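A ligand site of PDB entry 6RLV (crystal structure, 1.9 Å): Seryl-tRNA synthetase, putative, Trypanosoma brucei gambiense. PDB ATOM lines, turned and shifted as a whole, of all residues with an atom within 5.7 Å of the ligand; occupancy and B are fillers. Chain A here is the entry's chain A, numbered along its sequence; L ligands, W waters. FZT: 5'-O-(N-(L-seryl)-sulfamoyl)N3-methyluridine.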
ATOM      1  N   GLU A 248     -11.494  17.771 -16.992  1.00  0.00           N
ATOM      2  CA  GLU A 248     -10.140  18.042 -17.472  1.00  0.00           C
ATOM      3  C   GLU A 248      -9.869  19.433 -18.058  1.00  0.00           C
ATOM      4  O   GLU A 248      -8.729  19.879 -17.978  1.00  0.00           O
ATOM      5  CB  GLU A 248      -9.800  16.959 -18.523  1.00  0.00           C
ATOM      6  CG  GLU A 248      -8.340  16.821 -18.961  1.00  0.00           C
ATOM      7  CD  GLU A 248      -8.122  15.873 -20.122  1.00  0.00           C
ATOM      8  OE1 GLU A 248      -7.116  15.131 -20.118  1.00  0.00           O
ATOM      9  OE2 GLU A 248      -8.960  15.862 -21.064  1.00  0.00           O
ATOM     10  N   ALA A 263      -5.472  19.962 -23.456  1.00  0.00           N
ATOM     11  CA  ALA A 263      -4.972  18.947 -22.497  1.00  0.00           C
ATOM     12  C   ALA A 263      -3.832  18.156 -23.114  1.00  0.00           C
ATOM     13  O   ALA A 263      -3.143  17.394 -22.428  1.00  0.00           O
ATOM     14  CB  ALA A 263      -6.113  18.004 -22.110  1.00  0.00           C
ATOM     15  N   THR A 264      -3.628  18.322 -24.427  1.00  0.00           N
ATOM     16  CA  THR A 264      -2.601  17.634 -25.216  1.00  0.00           C
ATOM     17  C   THR A 264      -2.577  18.295 -26.603  1.00  0.00           C
ATOM     18  O   THR A 264      -3.622  18.766 -27.050  1.00  0.00           O
ATOM     19  CB  THR A 264      -2.966  16.118 -25.353  1.00  0.00           C
ATOM     20  OG1 THR A 264      -2.191  15.528 -26.404  1.00  0.00           O
ATOM     21  CG2 THR A 264      -4.489  15.870 -25.623  1.00  0.00           C
ATOM     22  N   GLU A 266      -2.626  16.695 -29.224  1.00  0.00           N
ATOM     23  CA  GLU A 266      -3.490  15.834 -30.044  1.00  0.00           C
ATOM     24  C   GLU A 266      -4.786  16.623 -30.391  1.00  0.00           C
ATOM     25  O   GLU A 266      -5.275  16.546 -31.508  1.00  0.00           O
ATOM     26  CB  GLU A 266      -3.860  14.556 -29.256  1.00  0.00           C
ATOM     27  CG  GLU A 266      -4.974  13.703 -29.896  1.00  0.00           C
ATOM     28  CD  GLU A 266      -5.780  12.853 -28.914  1.00  0.00           C
ATOM     29  OE1 GLU A 266      -5.288  12.578 -27.797  1.00  0.00           O
ATOM     30  OE2 GLU A 266      -6.907  12.473 -29.271  1.00  0.00           O
ATOM     31  N   ARG A 295      -4.427  20.366 -17.525  1.00  0.00           N
ATOM     32  CA  ARG A 295      -5.471  19.426 -17.115  1.00  0.00           C
ATOM     33  C   ARG A 295      -5.980  19.754 -15.722  1.00  0.00           C
ATOM     34  O   ARG A 295      -5.192  19.766 -14.788  1.00  0.00           O
ATOM     35  CB  ARG A 295      -4.938  17.984 -17.155  1.00  0.00           C
ATOM     36  CG  ARG A 295      -4.491  17.592 -18.548  1.00  0.00           C
ATOM     37  CD  ARG A 295      -4.175  16.126 -18.699  1.00  0.00           C
ATOM     38  NE  ARG A 295      -3.672  15.883 -20.042  1.00  0.00           N
ATOM     39  CZ  ARG A 295      -3.513  14.682 -20.583  1.00  0.00           C
ATOM     40  NH1 ARG A 295      -3.835  13.594 -19.883  1.00  0.00           N
ATOM     41  NH2 ARG A 295      -3.026  14.560 -21.803  1.00  0.00           N
ATOM     42  N   GLU A 297      -7.833  17.949 -13.780  1.00  0.00           N
ATOM     43  CA  GLU A 297      -7.716  16.704 -12.997  1.00  0.00           C
ATOM     44  C   GLU A 297      -8.721  16.657 -11.853  1.00  0.00           C
ATOM     45  O   GLU A 297      -8.356  16.340 -10.712  1.00  0.00           O
ATOM     46  CB  GLU A 297      -6.253  16.498 -12.529  1.00  0.00           C
ATOM     47  CG  GLU A 297      -5.325  16.374 -13.724  1.00  0.00           C
ATOM     48  CD  GLU A 297      -3.826  16.470 -13.522  1.00  0.00           C
ATOM     49  OE1 GLU A 297      -3.369  16.858 -12.418  1.00  0.00           O
ATOM     50  OE2 GLU A 297      -3.105  16.175 -14.505  1.00  0.00           O
ATOM     51  N   ILE A 308       6.058  16.354  -9.222  1.00  0.00           N
ATOM     52  CA  ILE A 308       5.603  16.785 -10.552  1.00  0.00           C
ATOM     53  C   ILE A 308       5.114  15.626 -11.420  1.00  0.00           C
ATOM     54  O   ILE A 308       4.989  15.779 -12.634  1.00  0.00           O
ATOM     55  CB  ILE A 308       6.645  17.684 -11.290  1.00  0.00           C
ATOM     56  CG1 ILE A 308       7.955  16.915 -11.629  1.00  0.00           C
ATOM     57  CG2 ILE A 308       6.929  18.969 -10.453  1.00  0.00           C
ATOM     58  CD1 ILE A 308       9.045  17.715 -12.488  1.00  0.00           C
ATOM     59  N   PHE A 309       4.772  14.501 -10.795  1.00  0.00           N
ATOM     60  CA  PHE A 309       4.279  13.328 -11.507  1.00  0.00           C
ATOM     61  C   PHE A 309       2.845  13.557 -12.023  1.00  0.00           C
ATOM     62  O   PHE A 309       2.528  13.133 -13.120  1.00  0.00           O
ATOM     63  CB  PHE A 309       4.369  12.076 -10.612  1.00  0.00           C
ATOM     64  CG  PHE A 309       3.946  10.818 -11.329  1.00  0.00           C
ATOM     65  CD1 PHE A 309       4.865  10.095 -12.084  1.00  0.00           C
ATOM     66  CD2 PHE A 309       2.632  10.366 -11.269  1.00  0.00           C
ATOM     67  CE1 PHE A 309       4.472   8.941 -12.783  1.00  0.00           C
ATOM     68  CE2 PHE A 309       2.238   9.219 -11.960  1.00  0.00           C
ATOM     69  CZ  PHE A 309       3.158   8.517 -12.718  1.00  0.00           C
ATOM     70  N   ARG A 310       1.989  14.188 -11.232  1.00  0.00           N
ATOM     71  CA  ARG A 310       0.610  14.462 -11.637  1.00  0.00           C
ATOM     72  C   ARG A 310       0.351  15.914 -11.334  1.00  0.00           C
ATOM     73  O   ARG A 310       0.212  16.294 -10.171  1.00  0.00           O
ATOM     74  CB  ARG A 310      -0.408  13.533 -10.936  1.00  0.00           C
ATOM     75  CG  ARG A 310      -1.759  13.570 -11.687  1.00  0.00           C
ATOM     76  CD  ARG A 310      -2.845  12.610 -11.207  1.00  0.00           C
ATOM     77  NE  ARG A 310      -2.345  11.512 -10.387  1.00  0.00           N
ATOM     78  CZ  ARG A 310      -2.038  10.290 -10.844  1.00  0.00           C
ATOM     79  NH1 ARG A 310      -2.172   9.995 -12.128  1.00  0.00           N
ATOM     80  NH2 ARG A 310      -1.578   9.362 -10.013  1.00  0.00           N
ATOM     81  N   VAL A 311       0.364  16.731 -12.365  1.00  0.00           N
ATOM     82  CA  VAL A 311       0.241  18.192 -12.221  1.00  0.00           C
ATOM     83  C   VAL A 311      -0.701  18.746 -13.263  1.00  0.00           C
ATOM     84  O   VAL A 311      -0.965  18.096 -14.270  1.00  0.00           O
ATOM     85  CB  VAL A 311       1.630  18.881 -12.275  1.00  0.00           C
ATOM     86  CG1 VAL A 311       2.421  18.642 -10.995  1.00  0.00           C
ATOM     87  CG2 VAL A 311       2.426  18.432 -13.508  1.00  0.00           C
ATOM     88  N   HIS A 312      -1.183  19.969 -13.052  1.00  0.00           N
ATOM     89  CA  HIS A 312      -2.106  20.578 -14.007  1.00  0.00           C
ATOM     90  C   HIS A 312      -1.427  21.069 -15.272  1.00  0.00           C
ATOM     91  O   HIS A 312      -2.089  21.195 -16.284  1.00  0.00           O
ATOM     92  CB  HIS A 312      -2.856  21.757 -13.373  1.00  0.00           C
ATOM     93  CG  HIS A 312      -3.620  21.406 -12.132  1.00  0.00           C
ATOM     94  ND1 HIS A 312      -4.761  20.624 -12.187  1.00  0.00           N
ATOM     95  CD2 HIS A 312      -3.393  21.760 -10.851  1.00  0.00           C
ATOM     96  CE1 HIS A 312      -5.188  20.518 -10.935  1.00  0.00           C
ATOM     97  NE2 HIS A 312      -4.411  21.195 -10.097  1.00  0.00           N
ATOM     98  N   PHE A 314       2.056  20.787 -17.842  1.00  0.00           N
ATOM     99  CA  PHE A 314       3.267  20.020 -18.196  1.00  0.00           C
ATOM    100  C   PHE A 314       3.515  20.039 -19.682  1.00  0.00           C
ATOM    101  O   PHE A 314       2.561  20.074 -20.451  1.00  0.00           O
ATOM    102  CB  PHE A 314       3.151  18.533 -17.706  1.00  0.00           C
ATOM    103  CG  PHE A 314       1.962  17.761 -18.240  1.00  0.00           C
ATOM    104  CD1 PHE A 314       2.099  16.899 -19.326  1.00  0.00           C
ATOM    105  CD2 PHE A 314       0.706  17.861 -17.625  1.00  0.00           C
ATOM    106  CE1 PHE A 314       1.011  16.150 -19.789  1.00  0.00           C
ATOM    107  CE2 PHE A 314      -0.389  17.137 -18.107  1.00  0.00           C
ATOM    108  CZ  PHE A 314      -0.231  16.282 -19.195  1.00  0.00           C
ATOM    109  N   LYS A 316       4.623  18.199 -23.214  1.00  0.00           N
ATOM    110  CA  LYS A 316       4.544  16.871 -23.810  1.00  0.00           C
ATOM    111  C   LYS A 316       4.876  16.985 -25.301  1.00  0.00           C
ATOM    112  O   LYS A 316       4.374  17.887 -25.997  1.00  0.00           O
ATOM    113  CB  LYS A 316       3.138  16.240 -23.565  1.00  0.00           C
ATOM    114  CG  LYS A 316       2.958  14.860 -24.237  1.00  0.00           C
ATOM    115  CD  LYS A 316       1.647  14.129 -23.837  1.00  0.00           C
ATOM    116  CE  LYS A 316       0.386  14.889 -24.220  1.00  0.00           C
ATOM    117  NZ  LYS A 316       0.384  15.247 -25.682  1.00  0.00           N
ATOM    118  N   GLU A 318       4.403  14.911 -28.717  1.00  0.00           N
ATOM    119  CA  GLU A 318       3.362  14.005 -29.188  1.00  0.00           C
ATOM    120  C   GLU A 318       3.598  13.492 -30.600  1.00  0.00           C
ATOM    121  O   GLU A 318       3.920  14.268 -31.475  1.00  0.00           O
ATOM    122  CB  GLU A 318       2.056  14.818 -29.197  1.00  0.00           C
ATOM    123  CG  GLU A 318       0.782  14.120 -29.636  1.00  0.00           C
ATOM    124  CD  GLU A 318       0.209  13.183 -28.598  1.00  0.00           C
ATOM    125  OE1 GLU A 318      -0.919  12.693 -28.830  1.00  0.00           O
ATOM    126  OE2 GLU A 318       0.832  12.976 -27.535  1.00  0.00           O
ATOM    127  N   GLU A 384       2.608   4.652 -15.746  1.00  0.00           N
ATOM    128  CA  GLU A 384       2.329   5.089 -17.105  1.00  0.00           C
ATOM    129  C   GLU A 384       3.136   6.342 -17.509  1.00  0.00           C
ATOM    130  O   GLU A 384       3.084   7.367 -16.831  1.00  0.00           O
ATOM    131  CB  GLU A 384       0.815   5.372 -17.217  1.00  0.00           C
ATOM    132  CG  GLU A 384       0.388   5.863 -18.597  1.00  0.00           C
ATOM    133  CD  GLU A 384      -0.999   6.443 -18.641  1.00  0.00           C
ATOM    134  OE1 GLU A 384      -1.804   6.173 -17.718  1.00  0.00           O
ATOM    135  OE2 GLU A 384      -1.302   7.174 -19.607  1.00  0.00           O
ATOM    136  N   LEU A 385       3.875   6.257 -18.647  1.00  0.00           N
ATOM    137  CA  LEU A 385       4.576   7.407 -19.239  1.00  0.00           C
ATOM    138  C   LEU A 385       3.970   7.747 -20.588  1.00  0.00           C
ATOM    139  O   LEU A 385       4.097   8.878 -21.063  1.00  0.00           O
ATOM    140  CB  LEU A 385       6.075   7.076 -19.488  1.00  0.00           C
ATOM    141  CG  LEU A 385       7.046   7.070 -18.296  1.00  0.00           C
ATOM    142  CD1 LEU A 385       8.497   7.309 -18.752  1.00  0.00           C
ATOM    143  CD2 LEU A 385       6.688   8.128 -17.267  1.00  0.00           C
ATOM    144  N   VAL A 386       3.394   6.731 -21.261  1.00  0.00           N
ATOM    145  CA  VAL A 386       2.939   6.847 -22.642  1.00  0.00           C
ATOM    146  C   VAL A 386       1.646   6.114 -22.887  1.00  0.00           C
ATOM    147  O   VAL A 386       1.489   5.011 -22.412  1.00  0.00           O
ATOM    148  CB  VAL A 386       4.049   6.187 -23.574  1.00  0.00           C
ATOM    149  CG1 VAL A 386       3.533   5.916 -25.001  1.00  0.00           C
ATOM    150  CG2 VAL A 386       5.357   7.008 -23.609  1.00  0.00           C
ATOM    151  N   SER A 387       0.810   6.681 -23.764  1.00  0.00           N
ATOM    152  CA  SER A 387      -0.361   6.016 -24.334  1.00  0.00           C
ATOM    153  C   SER A 387      -0.267   6.218 -25.846  1.00  0.00           C
ATOM    154  O   SER A 387      -0.023   7.339 -26.297  1.00  0.00           O
ATOM    155  CB  SER A 387      -1.672   6.615 -23.816  1.00  0.00           C
ATOM    156  OG  SER A 387      -1.991   6.163 -22.517  1.00  0.00           O
ATOM    157  N   CYS A 388      -0.446   5.123 -26.617  1.00  0.00           N
ATOM    158  CA  CYS A 388      -0.432   5.138 -28.097  1.00  0.00           C
ATOM    159  C   CYS A 388      -1.726   4.503 -28.520  1.00  0.00           C
ATOM    160  O   CYS A 388      -1.975   3.344 -28.179  1.00  0.00           O
ATOM    161  CB  CYS A 388       0.742   4.333 -28.675  1.00  0.00           C
ATOM    162  SG  CYS A 388       2.325   5.182 -28.654  1.00  0.00           S
ATOM    163  N   ASN A 423      -2.585   8.758 -32.380  1.00  0.00           N
ATOM    164  CA  ASN A 423      -1.849   9.673 -31.505  1.00  0.00           C
ATOM    165  C   ASN A 423      -1.101   8.835 -30.489  1.00  0.00           C
ATOM    166  O   ASN A 423      -1.560   7.757 -30.085  1.00  0.00           O
ATOM    167  CB  ASN A 423      -2.770  10.706 -30.830  1.00  0.00           C
ATOM    168  CG  ASN A 423      -3.713  10.098 -29.840  1.00  0.00           C
ATOM    169  OD1 ASN A 423      -3.359   9.879 -28.682  1.00  0.00           O
ATOM    170  ND2 ASN A 423      -4.918   9.769 -30.279  1.00  0.00           N
ATOM    171  N   GLY A 424       0.063   9.310 -30.094  1.00  0.00           N
ATOM    172  CA  GLY A 424       0.861   8.576 -29.130  1.00  0.00           C
ATOM    173  C   GLY A 424       1.857   9.468 -28.437  1.00  0.00           C
ATOM    174  O   GLY A 424       2.570  10.235 -29.091  1.00  0.00           O
ATOM    175  N   THR A 425       1.946   9.340 -27.122  1.00  0.00           N
ATOM    176  CA  THR A 425       2.934  10.139 -26.389  1.00  0.00           C
ATOM    177  C   THR A 425       4.315   9.735 -26.873  1.00  0.00           C
ATOM    178  O   THR A 425       4.592   8.545 -27.001  1.00  0.00           O
ATOM    179  CB  THR A 425       2.869   9.794 -24.884  1.00  0.00           C
ATOM    180  OG1 THR A 425       1.520   9.808 -24.467  1.00  0.00           O
ATOM    181  CG2 THR A 425       3.675  10.765 -24.001  1.00  0.00           C
ATOM    182  N   LEU A 426       5.212  10.722 -27.043  1.00  0.00           N
ATOM    183  CA  LEU A 426       6.625  10.393 -27.269  1.00  0.00           C
ATOM    184  C   LEU A 426       7.285  10.666 -25.921  1.00  0.00           C
ATOM    185  O   LEU A 426       7.915   9.784 -25.332  1.00  0.00           O
ATOM    186  CB  LEU A 426       7.253  11.215 -28.415  1.00  0.00           C
ATOM    187  CG  LEU A 426       8.694  10.841 -28.826  1.00  0.00           C
ATOM    188  CD1 LEU A 426       9.721  11.538 -27.967  1.00  0.00           C
ATOM    189  CD2 LEU A 426       8.904   9.287 -28.894  1.00  0.00           C
ATOM    190  N   ALA A 428       6.253  12.681 -22.133  1.00  0.00           N
ATOM    191  CA  ALA A 428       5.537  13.533 -21.169  1.00  0.00           C
ATOM    192  C   ALA A 428       6.719  13.977 -20.297  1.00  0.00           C
ATOM    193  O   ALA A 428       7.320  13.164 -19.576  1.00  0.00           O
ATOM    194  CB  ALA A 428       4.529  12.725 -20.379  1.00  0.00           C
ATOM    195  N   ILE A 429       7.135  15.233 -20.463  1.00  0.00           N
ATOM    196  CA  ILE A 429       8.384  15.755 -19.893  1.00  0.00           C
ATOM    197  C   ILE A 429       8.535  15.619 -18.381  1.00  0.00           C
ATOM    198  O   ILE A 429       9.570  15.093 -17.946  1.00  0.00           O
ATOM    199  CB  ILE A 429       8.641  17.227 -20.379  1.00  0.00           C
ATOM    200  CG1 ILE A 429       8.608  17.343 -21.934  1.00  0.00           C
ATOM    201  CG2 ILE A 429       9.914  17.833 -19.753  1.00  0.00           C
ATOM    202  CD1 ILE A 429       9.651  16.641 -22.761  1.00  0.00           C
ATOM    203  N   THR A 430       7.572  16.103 -17.576  1.00  0.00           N
ATOM    204  CA  THR A 430       7.751  16.047 -16.103  1.00  0.00           C
ATOM    205  C   THR A 430       7.792  14.612 -15.578  1.00  0.00           C
ATOM    206  O   THR A 430       8.600  14.315 -14.684  1.00  0.00           O
ATOM    207  CB  THR A 430       6.728  16.914 -15.315  1.00  0.00           C
ATOM    208  OG1 THR A 430       5.424  16.320 -15.339  1.00  0.00           O
ATOM    209  CG2 THR A 430       6.680  18.369 -15.793  1.00  0.00           C
ATOM    210  N   ARG A 431       6.945  13.720 -16.117  1.00  0.00           N
ATOM    211  CA  ARG A 431       6.959  12.302 -15.681  1.00  0.00           C
ATOM    212  C   ARG A 431       8.228  11.614 -16.069  1.00  0.00           C
ATOM    213  O   ARG A 431       8.709  10.796 -15.288  1.00  0.00           O
ATOM    214  CB  ARG A 431       5.784  11.521 -16.244  1.00  0.00           C
ATOM    215  CG  ARG A 431       4.531  11.835 -15.545  1.00  0.00           C
ATOM    216  CD  ARG A 431       3.515  10.749 -15.739  1.00  0.00           C
ATOM    217  NE  ARG A 431       2.325  11.201 -15.041  1.00  0.00           N
ATOM    218  CZ  ARG A 431       1.184  10.561 -15.012  1.00  0.00           C
ATOM    219  NH1 ARG A 431       1.046   9.400 -15.658  1.00  0.00           N
ATOM    220  NH2 ARG A 431       0.179  11.045 -14.322  1.00  0.00           N
HETATM  221  C3U FZT L   1       1.905  15.216 -15.573  1.00  0.00           C
HETATM  222  N3  FZT L   1       0.965  14.344 -16.298  1.00  0.00           N
HETATM  223  C4  FZT L   1      -0.360  14.280 -15.848  1.00  0.00           C
HETATM  224  O4  FZT L   1      -0.668  14.862 -14.812  1.00  0.00           O
HETATM  225  C5  FZT L   1      -1.239  13.469 -16.632  1.00  0.00           C
HETATM  226  C6  FZT L   1      -0.776  12.786 -17.699  1.00  0.00           C
HETATM  227  N1  FZT L   1       0.553  12.832 -18.049  1.00  0.00           N
HETATM  228  C1' FZT L   1       1.111  11.961 -19.107  1.00  0.00           C
HETATM  229  O4' FZT L   1       0.529  12.295 -20.351  1.00  0.00           O
HETATM  230  C4' FZT L   1       0.504  11.105 -21.145  1.00  0.00           C
HETATM  231  C5' FZT L   1      -0.471  11.288 -22.290  1.00  0.00           C
HETATM  232  O5' FZT L   1      -1.787  11.561 -21.717  1.00  0.00           O
HETATM  233  S   FZT L   1      -3.022  10.658 -22.167  1.00  0.00           S
HETATM  234  O1S FZT L   1      -4.162  11.393 -21.757  1.00  0.00           O
HETATM  235  O2S FZT L   1      -2.763   9.351 -21.664  1.00  0.00           O
HETATM  236  N3S FZT L   1      -2.913  10.578 -23.751  1.00  0.00           N
HETATM  237  C   FZT L   1      -2.809  11.709 -24.608  1.00  0.00           C
HETATM  238  O   FZT L   1      -2.885  12.854 -24.152  1.00  0.00           O
HETATM  239  CA  FZT L   1      -2.636  11.361 -26.058  1.00  0.00           C
HETATM  240  N   FZT L   1      -2.755  12.566 -26.900  1.00  0.00           N
HETATM  241  CB  FZT L   1      -1.296  10.651 -26.250  1.00  0.00           C
HETATM  242  OG  FZT L   1      -0.221  11.404 -25.693  1.00  0.00           O
HETATM  243  C3' FZT L   1       0.157  10.012 -20.152  1.00  0.00           C
HETATM  244  O3' FZT L   1       0.555   8.735 -20.619  1.00  0.00           O
HETATM  245  C2' FZT L   1       0.903  10.450 -18.883  1.00  0.00           C
HETATM  246  O2' FZT L   1       2.172   9.817 -18.795  1.00  0.00           O
HETATM  247  C2  FZT L   1       1.468  13.626 -17.372  1.00  0.00           C
HETATM  248  O2  FZT L   1       2.648  13.676 -17.672  1.00  0.00           O
HETATM  249  O   HOH W   1      -4.474   8.134 -19.241  1.00  0.00           O
HETATM  250  O   HOH W   2      -6.487  13.397 -22.490  1.00  0.00           O
HETATM  251  O   HOH W   3      -4.394   8.375 -24.766  1.00  0.00           O
HETATM  252  O   HOH W   4       4.824  15.176 -17.728  1.00  0.00           O
HETATM  253  O   HOH W   5      -4.984   7.025 -22.279  1.00  0.00           O
HETATM  254  O   HOH W   6      -3.129  10.249 -18.148  1.00  0.00           O
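Water W4 lies within hydrogen-bond range of an oxygen (O2) of the ligand (2.6 Å), the side-chain hydroxyl of Thr 430 (2.7 Å) and the backbone NH of Arg 431 (3.0 Å).
Water W2 bridges the side-chain carboxylate (OE1) of Glu 248 (3.0 Å) and an oxygen (O1S) of the ligand (3.2 Å).
Water W1 lies within hydrogen-bond range of an oxygen (O2S) of the ligand (3.2 Å) and the side-chain carboxylate of Glu 384 (3.3 Å).
Water W5 bridges OG of Ser 387 and O2S of the ligand.
The side-chain amino group (NZ) of Lys 316 is in salt-bridge range of the side-chain carboxylate (OE2) of Glu 318.
N of Glu 266 lies close to OG1 of Thr 264, at 3.1 Å.
The side-chain amide oxygen (OD1) of Asn 423 sits close to the side-chain carboxylate (OE1) of Glu 266 (3.4 Å).
The guanidinium group of Arg 295 lies within hydrogen-bond range of the backbone carbonyl oxygen of Ala 263 (2.9 Å).
OE1 of Glu 248 lies within salt-bridge range of NE of Arg 295, at 3.5 Å.
O of Arg 295 is in hydrogen-bond range of ND1 of His 312.
The side-chain amino group (NZ) of Lys 316 is in hydrogen-bond range of the side-chain hydroxyl (OG1) of Thr 264.
The backbone carbonyl oxygen of Ile 308 sits at hydrogen-bond distance from the side-chain hydroxyl of Thr 430 (2.8 Å).
The side-chain carboxylate (OE2) of Glu 297 lies close to an oxygen (O4) of the ligand (2.8 Å).
Residues that only touch the ligand: Phe 309 (3.3 Å), Arg 310 (3.4 Å), Phe 314 (3.5 Å), Lys 316 (3.8 Å), Val 386 (3.5 Å), Gly 424 (3.9 Å), Ala 428 (3.4 Å) and Thr 430 (3.7 Å).
Hydrophobic or aromatic side chains within 4 Å of the ligand: Val 311, Phe 314 and Ala 428.
Of the 27 residues printed, 20 come within 4 Å of the ligand.
O2' of the ligand lies within hydrogen-bond range of O of Glu 384 (3.3 Å).
The side-chain carboxylate (OE2) of Glu 384 sits at hydrogen-bond distance from an oxygen (O3') of the ligand (2.6 Å).
OE1 of Glu 318 is in salt-bridge range of N of the ligand (2.7 Å).
An oxygen (OG) of the ligand lies within hydrogen-bond range of the backbone NH (N) of Thr 425.
An oxygen (OG) of the ligand lies within hydrogen-bond range of the side-chain hydroxyl (OG1) of Thr 425 (2.7 Å).
The side-chain carboxylate of Glu 266 lies within salt-bridge range of a nitrogen (N) of the ligand.
O of the ligand is in hydrogen-bond range of NH2 of Arg 295.
The side-chain hydroxyl (OG1) of Thr 264 is in hydrogen-bond range of a nitrogen (N) of the ligand.
The side-chain amide oxygen of Asn 423 lies close to a nitrogen (N) of the ligand.
O of Leu 385 sits at hydrogen-bond distance from O2' of the ligand, 3.1 Å away.
N of Val 311 sits at hydrogen-bond distance from O4 of the ligand.
An oxygen (O2') of the ligand is in hydrogen-bond range of the guanidinium group (NH1) of Arg 431 (3.4 Å).
O2S of the ligand lies within hydrogen-bond range of OG of Ser 387.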
